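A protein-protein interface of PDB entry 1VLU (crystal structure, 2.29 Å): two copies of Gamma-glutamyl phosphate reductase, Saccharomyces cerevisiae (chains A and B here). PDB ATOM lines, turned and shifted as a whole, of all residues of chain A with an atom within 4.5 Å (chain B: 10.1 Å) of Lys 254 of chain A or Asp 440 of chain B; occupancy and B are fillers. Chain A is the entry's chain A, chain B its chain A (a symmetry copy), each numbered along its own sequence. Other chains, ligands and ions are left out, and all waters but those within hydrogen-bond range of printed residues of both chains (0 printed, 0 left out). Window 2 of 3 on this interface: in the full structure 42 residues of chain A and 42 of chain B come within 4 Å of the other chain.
O of Gly 441 of chain B sits at hydrogen-bond distance from NH1 of Arg 257 of chain A (2.5 Å). NZ of Lys 254 of chain A is in salt-bridge range of OD1 of Asp 440 of chain B, 3.5 Å away. The backbone carbonyl oxygen of Asn 395 of chain A sits at hydrogen-bond distance from the backbone NH of Asp 440 of chain B (3.5 Å). N of Gly 441 of chain B sits at hydrogen-bond distance from O of Asn 395 of chain A (2.6 Å).
No position is printed for both chains. Of the 9 pairs that touch across the chains among the printed residues, none has its exchanged pair printed and touching as well.
Of the 11 printed residues of chain A, 4 touch a printed residue of chain B. Of the 12 printed residues of chain B, 5 touch a printed residue of chain A. Hydrophobic or aromatic side chains of chain B that line the printed part of chain A: Val 443.
The side-chain carboxylate (OE2) of Glu 375 of chain A lies within salt-bridge range of the side-chain amino group (NZ) of Lys 254 of chain A (2.4 Å). The side-chain amide oxygen (OE1) of Gln 442 of chain B lies within hydrogen-bond range of the backbone NH (N) of Asp 440 of chain B (2.6 Å). The backbone carbonyl oxygen (O) of Asp 116 of chain B is in hydrogen-bond range of the side-chain amide nitrogen (NE2) of Gln 442 of chain B (3.3 Å). The side-chain carboxylate (OD1) of Asp 251 of chain A lies within hydrogen-bond range of the backbone NH (N) of Lys 254 of chain A.
Of chain B, only Asp 440 (3.5 Å) and Gly 441 (3.8 Å) come within 4 Å of Lys 254 of chain A. Of chain A, only Lys 254 (3.5 Å) and Asn 395 (3.5 Å) come within 4 Å of Asp 440 of chain B. No residue of chain B comes within 4 Å of Asp 251 of chain A. No residue of chain B comes within 4 Å of Ile 253 of chain A. No residue of chain B comes within 4 Å of Ala 255 of chain A. Ile 258 of chain A touches just one residue of chain B: Val 443 (3.7 Å). Printed residues of chain A within 4 Å of Gly 441 of chain B: Lys 254, Arg 257 and Asn 395. Of the printed residues of chain B, Asn 395 of chain A touches Gly 439, Asp 440, Gly 441 and Gln 442. Lys 256 of chain A touches none of the printed residues of chain B. Gly 117 of chain B touches none of the printed residues of chain A. The nearest residue of chain B that does not touch Lys 254 of chain A is Val 443 of chain B (5.9 Å). The nearest printed residue of chain A that does not touch Gln 442 of chain B is Arg 257 of chain A (4.01 Å).
Among the printed residues, pairs that only touch across the chains: Lys 254 of chain A with Gly 441 of chain B, Arg 257 of chain A with Val 443 of chain B, Ile 258 of chain A with Val 443 of chain B, Asn 395 of chain A with Gly 439 of chain B and Asn 395 of chain A with Gln 442 of chain B.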
ATOM      1  N   ASP A 251      17.244  -2.959  -0.351  1.00  0.00           N
ATOM      2  CA  ASP A 251      17.927  -3.824  -1.301  1.00  0.00           C
ATOM      3  C   ASP A 251      17.126  -5.121  -1.403  1.00  0.00           C
ATOM      4  O   ASP A 251      16.751  -5.712  -0.372  1.00  0.00           O
ATOM      5  CB  ASP A 251      19.344  -4.111  -0.820  1.00  0.00           C
ATOM      6  CG  ASP A 251      20.130  -4.974  -1.793  1.00  0.00           C
ATOM      7  OD1 ASP A 251      19.806  -6.177  -1.941  1.00  0.00           O
ATOM      8  OD2 ASP A 251      21.085  -4.444  -2.400  1.00  0.00           O
ATOM      9  N   LEU A 252      16.866  -5.554  -2.635  1.00  0.00           N
ATOM     10  CA  LEU A 252      15.995  -6.700  -2.900  1.00  0.00           C
ATOM     11  C   LEU A 252      16.619  -8.055  -2.538  1.00  0.00           C
ATOM     12  O   LEU A 252      15.924  -8.933  -2.013  1.00  0.00           O
ATOM     13  CB  LEU A 252      15.505  -6.690  -4.355  1.00  0.00           C
ATOM     14  CG  LEU A 252      14.628  -7.836  -4.894  1.00  0.00           C
ATOM     15  CD1 LEU A 252      13.174  -7.801  -4.386  1.00  0.00           C
ATOM     16  CD2 LEU A 252      14.664  -7.815  -6.395  1.00  0.00           C
ATOM     17  N   ILE A 253      17.911  -8.221  -2.813  1.00  0.00           N
ATOM     18  CA  ILE A 253      18.635  -9.432  -2.421  1.00  0.00           C
ATOM     19  C   ILE A 253      18.653  -9.568  -0.890  1.00  0.00           C
ATOM     20  O   ILE A 253      18.310 -10.631  -0.364  1.00  0.00           O
ATOM     21  CB  ILE A 253      20.082  -9.464  -2.998  1.00  0.00           C
ATOM     22  CG1 ILE A 253      20.048  -9.553  -4.532  1.00  0.00           C
ATOM     23  CG2 ILE A 253      20.897 -10.618  -2.377  1.00  0.00           C
ATOM     24  CD1 ILE A 253      21.175  -8.781  -5.219  1.00  0.00           C
ATOM     25  N   LYS A 254      19.027  -8.495  -0.185  1.00  0.00           N
ATOM     26  CA  LYS A 254      18.975  -8.477   1.287  1.00  0.00           C
ATOM     27  C   LYS A 254      17.567  -8.691   1.824  1.00  0.00           C
ATOM     28  O   LYS A 254      17.371  -9.459   2.753  1.00  0.00           O
ATOM     29  CB  LYS A 254      19.522  -7.178   1.854  1.00  0.00           C
ATOM     30  CG  LYS A 254      21.007  -7.027   1.762  1.00  0.00           C
ATOM     31  CD  LYS A 254      21.386  -5.689   2.360  1.00  0.00           C
ATOM     32  CE  LYS A 254      22.674  -5.184   1.772  1.00  0.00           C
ATOM     33  NZ  LYS A 254      22.701  -3.707   1.811  1.00  0.00           N
ATOM     34  N   ALA A 255      16.590  -8.006   1.240  1.00  0.00           N
ATOM     35  CA  ALA A 255      15.202  -8.127   1.679  1.00  0.00           C
ATOM     36  C   ALA A 255      14.705  -9.573   1.588  1.00  0.00           C
ATOM     37  O   ALA A 255      13.936 -10.023   2.438  1.00  0.00           O
ATOM     38  CB  ALA A 255      14.297  -7.198   0.856  1.00  0.00           C
ATOM     39  N   LYS A 256      15.151 -10.280   0.549  1.00  0.00           N
ATOM     40  CA  LYS A 256      14.774 -11.666   0.314  1.00  0.00           C
ATOM     41  C   LYS A 256      15.406 -12.615   1.311  1.00  0.00           C
ATOM     42  O   LYS A 256      14.719 -13.473   1.856  1.00  0.00           O
ATOM     43  CB  LYS A 256      15.150 -12.098  -1.107  1.00  0.00           C
ATOM     44  CG  LYS A 256      14.109 -11.766  -2.156  1.00  0.00           C
ATOM     45  CD  LYS A 256      14.621 -12.120  -3.529  1.00  0.00           C
ATOM     46  CE  LYS A 256      13.586 -11.780  -4.590  1.00  0.00           C
ATOM     47  NZ  LYS A 256      14.072 -12.019  -5.990  1.00  0.00           N
ATOM     48  N   ARG A 257      16.709 -12.469   1.537  1.00  0.00           N
ATOM     49  CA  ARG A 257      17.414 -13.350   2.455  1.00  0.00           C
ATOM     50  C   ARG A 257      16.990 -13.105   3.905  1.00  0.00           C
ATOM     51  O   ARG A 257      16.591 -14.042   4.596  1.00  0.00           O
ATOM     52  CB  ARG A 257      18.933 -13.269   2.253  1.00  0.00           C
ATOM     53  CG  ARG A 257      19.640 -12.025   2.805  1.00  0.00           C
ATOM     54  CD  ARG A 257      21.059 -11.922   2.239  1.00  0.00           C
ATOM     55  NE  ARG A 257      21.623 -13.250   1.986  1.00  0.00           N
ATOM     56  CZ  ARG A 257      22.410 -13.923   2.824  1.00  0.00           C
ATOM     57  NH1 ARG A 257      22.772 -13.399   3.988  1.00  0.00           N
ATOM     58  NH2 ARG A 257      22.846 -15.131   2.486  1.00  0.00           N
ATOM     59  N   ILE A 258      17.022 -11.849   4.345  1.00  0.00           N
ATOM     60  CA  ILE A 258      16.585 -11.486   5.693  1.00  0.00           C
ATOM     61  C   ILE A 258      15.179 -12.015   5.983  1.00  0.00           C
ATOM     62  O   ILE A 258      14.965 -12.658   7.012  1.00  0.00           O
ATOM     63  CB  ILE A 258      16.705  -9.969   5.951  1.00  0.00           C
ATOM     64  CG1 ILE A 258      18.178  -9.598   6.099  1.00  0.00           C
ATOM     65  CG2 ILE A 258      15.896  -9.532   7.199  1.00  0.00           C
ATOM     66  CD1 ILE A 258      18.453  -8.125   5.938  1.00  0.00           C
ATOM     67  N   VAL A 373      14.808  -3.098   6.594  1.00  0.00           N
ATOM     68  CA  VAL A 373      15.655  -3.369   5.445  1.00  0.00           C
ATOM     69  C   VAL A 373      15.612  -2.112   4.575  1.00  0.00           C
ATOM     70  O   VAL A 373      14.571  -1.757   4.020  1.00  0.00           O
ATOM     71  CB  VAL A 373      15.191  -4.637   4.671  1.00  0.00           C
ATOM     72  CG1 VAL A 373      16.189  -5.001   3.599  1.00  0.00           C
ATOM     73  CG2 VAL A 373      14.992  -5.814   5.638  1.00  0.00           C
ATOM     74  N   GLU A 375      18.563   0.854   2.359  1.00  0.00           N
ATOM     75  CA  GLU A 375      19.880   1.441   2.075  1.00  0.00           C
ATOM     76  C   GLU A 375      19.914   2.923   2.459  1.00  0.00           C
ATOM     77  O   GLU A 375      20.969   3.554   2.458  1.00  0.00           O
ATOM     78  CB  GLU A 375      20.249   1.275   0.593  1.00  0.00           C
ATOM     79  CG  GLU A 375      20.438  -0.183   0.136  1.00  0.00           C
ATOM     80  CD  GLU A 375      21.386  -0.988   1.031  1.00  0.00           C
ATOM     81  OE1 GLU A 375      22.568  -0.597   1.168  1.00  0.00           O
ATOM     82  OE2 GLU A 375      20.946  -2.021   1.592  1.00  0.00           O
ATOM     83  N   ASN A 395      19.368  -4.119   8.375  1.00  0.00           N
ATOM     84  CA  ASN A 395      19.974  -5.017   7.382  1.00  0.00           C
ATOM     85  C   ASN A 395      20.587  -6.300   7.965  1.00  0.00           C
ATOM     86  O   ASN A 395      21.627  -6.748   7.499  1.00  0.00           O
ATOM     87  CB  ASN A 395      21.001  -4.283   6.504  1.00  0.00           C
ATOM     88  CG  ASN A 395      20.363  -3.277   5.561  1.00  0.00           C
ATOM     89  OD1 ASN A 395      19.202  -3.413   5.162  1.00  0.00           O
ATOM     90  ND2 ASN A 395      21.130  -2.261   5.191  1.00  0.00           N
ATOM     91  N   ASP B 115      30.658 -10.211  13.938  1.00  0.00           N
ATOM     92  CA  ASP B 115      31.142 -10.808  12.694  1.00  0.00           C
ATOM     93  C   ASP B 115      31.543  -9.607  11.819  1.00  0.00           C
ATOM     94  O   ASP B 115      31.241  -8.466  12.172  1.00  0.00           O
ATOM     95  CB  ASP B 115      30.029 -11.684  12.070  1.00  0.00           C
ATOM     96  CG  ASP B 115      30.363 -12.201  10.672  1.00  0.00           C
ATOM     97  OD1 ASP B 115      31.457 -12.789  10.462  1.00  0.00           O
ATOM     98  OD2 ASP B 115      29.493 -12.031   9.781  1.00  0.00           O
ATOM     99  N   ASP B 116      32.250  -9.840  10.715  1.00  0.00           N
ATOM    100  CA  ASP B 116      32.675  -8.748   9.827  1.00  0.00           C
ATOM    101  C   ASP B 116      31.464  -7.963   9.302  1.00  0.00           C
ATOM    102  O   ASP B 116      30.551  -8.545   8.707  1.00  0.00           O
ATOM    103  CB  ASP B 116      33.519  -9.287   8.670  1.00  0.00           C
ATOM    104  N   GLY B 117      31.450  -6.654   9.554  1.00  0.00           N
ATOM    105  CA  GLY B 117      30.329  -5.787   9.173  1.00  0.00           C
ATOM    106  C   GLY B 117      29.011  -6.110   9.867  1.00  0.00           C
ATOM    107  O   GLY B 117      27.950  -5.727   9.392  1.00  0.00           O
ATOM    108  N   LEU B 118      29.083  -6.834  10.980  1.00  0.00           N
ATOM    109  CA  LEU B 118      27.927  -7.111  11.823  1.00  0.00           C
ATOM    110  C   LEU B 118      28.296  -6.726  13.256  1.00  0.00           C
ATOM    111  O   LEU B 118      29.127  -7.378  13.888  1.00  0.00           O
ATOM    112  CB  LEU B 118      27.517  -8.591  11.717  1.00  0.00           C
ATOM    113  CG  LEU B 118      26.266  -9.123  12.445  1.00  0.00           C
ATOM    114  CD1 LEU B 118      24.980  -8.603  11.816  1.00  0.00           C
ATOM    115  CD2 LEU B 118      26.286 -10.657  12.439  1.00  0.00           C
ATOM    116  N   THR B 119      27.685  -5.655  13.751  1.00  0.00           N
ATOM    117  CA  THR B 119      28.028  -5.089  15.047  1.00  0.00           C
ATOM    118  C   THR B 119      26.786  -4.900  15.909  1.00  0.00           C
ATOM    119  O   THR B 119      25.755  -4.439  15.426  1.00  0.00           O
ATOM    120  CB  THR B 119      28.755  -3.741  14.862  1.00  0.00           C
ATOM    121  OG1 THR B 119      29.835  -3.913  13.932  1.00  0.00           O
ATOM    122  CG2 THR B 119      29.322  -3.223  16.185  1.00  0.00           C
ATOM    123  N   ILE B 437      21.376  -4.157  16.183  1.00  0.00           N
ATOM    124  CA  ILE B 437      22.302  -4.920  15.361  1.00  0.00           C
ATOM    125  C   ILE B 437      22.280  -4.288  13.984  1.00  0.00           C
ATOM    126  O   ILE B 437      21.213  -4.028  13.405  1.00  0.00           O
ATOM    127  CB  ILE B 437      21.963  -6.435  15.321  1.00  0.00           C
ATOM    128  CG1 ILE B 437      22.041  -7.006  16.748  1.00  0.00           C
ATOM    129  CG2 ILE B 437      22.878  -7.154  14.361  1.00  0.00           C
ATOM    130  CD1 ILE B 437      22.160  -8.542  16.890  1.00  0.00           C
ATOM    131  N   ARG B 438      23.469  -3.997  13.489  1.00  0.00           N
ATOM    132  CA  ARG B 438      23.635  -3.302  12.236  1.00  0.00           C
ATOM    133  C   ARG B 438      24.532  -4.169  11.420  1.00  0.00           C
ATOM    134  O   ARG B 438      25.726  -4.254  11.690  1.00  0.00           O
ATOM    135  CB  ARG B 438      24.276  -1.933  12.461  1.00  0.00           C
ATOM    136  CG  ARG B 438      23.478  -1.023  13.377  1.00  0.00           C
ATOM    137  CD  ARG B 438      24.250   0.257  13.610  1.00  0.00           C
ATOM    138  NE  ARG B 438      23.516   1.211  14.418  1.00  0.00           N
ATOM    139  CZ  ARG B 438      23.206   2.442  14.020  1.00  0.00           C
ATOM    140  NH1 ARG B 438      23.575   2.877  12.821  1.00  0.00           N
ATOM    141  NH2 ARG B 438      22.525   3.245  14.827  1.00  0.00           N
ATOM    142  N   GLY B 439      23.948  -4.842  10.436  1.00  0.00           N
ATOM    143  CA  GLY B 439      24.699  -5.711   9.546  1.00  0.00           C
ATOM    144  C   GLY B 439      24.558  -5.278   8.102  1.00  0.00           C
ATOM    145  O   GLY B 439      24.047  -4.199   7.824  1.00  0.00           O
ATOM    146  N   ASP B 440      25.023  -6.122   7.186  1.00  0.00           N
ATOM    147  CA  ASP B 440      24.862  -5.873   5.754  1.00  0.00           C
ATOM    148  C   ASP B 440      24.264  -7.078   5.029  1.00  0.00           C
ATOM    149  O   ASP B 440      24.803  -7.544   4.029  1.00  0.00           O
ATOM    150  CB  ASP B 440      26.188  -5.452   5.109  1.00  0.00           C
ATOM    151  CG  ASP B 440      25.988  -4.442   3.986  1.00  0.00           C
ATOM    152  OD1 ASP B 440      25.199  -3.482   4.203  1.00  0.00           O
ATOM    153  OD2 ASP B 440      26.604  -4.606   2.898  1.00  0.00           O
ATOM    154  N   GLY B 441      23.154  -7.587   5.558  1.00  0.00           N
ATOM    155  CA  GLY B 441      22.404  -8.662   4.921  1.00  0.00           C
ATOM    156  C   GLY B 441      22.673 -10.034   5.497  1.00  0.00           C
ATOM    157  O   GLY B 441      22.387 -11.032   4.851  1.00  0.00           O
ATOM    158  N   GLN B 442      23.219 -10.079   6.713  1.00  0.00           N
ATOM    159  CA  GLN B 442      23.573 -11.356   7.348  1.00  0.00           C
ATOM    160  C   GLN B 442      22.360 -12.011   7.982  1.00  0.00           C
ATOM    161  O   GLN B 442      21.526 -11.348   8.617  1.00  0.00           O
ATOM    162  CB  GLN B 442      24.689 -11.206   8.399  1.00  0.00           C
ATOM    163  CG  GLN B 442      26.058 -10.814   7.848  1.00  0.00           C
ATOM    164  CD  GLN B 442      26.256  -9.313   7.824  1.00  0.00           C
ATOM    165  OE1 GLN B 442      25.323  -8.548   8.094  1.00  0.00           O
ATOM    166  NE2 GLN B 442      27.471  -8.879   7.507  1.00  0.00           N
ATOM    167  N   VAL B 443      22.295 -13.327   7.812  1.00  0.00           N
ATOM    168  CA  VAL B 443      21.169 -14.131   8.274  1.00  0.00           C
ATOM    169  C   VAL B 443      21.634 -15.228   9.237  1.00  0.00           C
ATOM    170  O   VAL B 443      22.809 -15.599   9.240  1.00  0.00           O
ATOM    171  CB  VAL B 443      20.379 -14.714   7.079  1.00  0.00           C
ATOM    172  CG1 VAL B 443      19.588 -13.605   6.399  1.00  0.00           C
ATOM    173  CG2 VAL B 443      21.313 -15.444   6.074  1.00  0.00           C
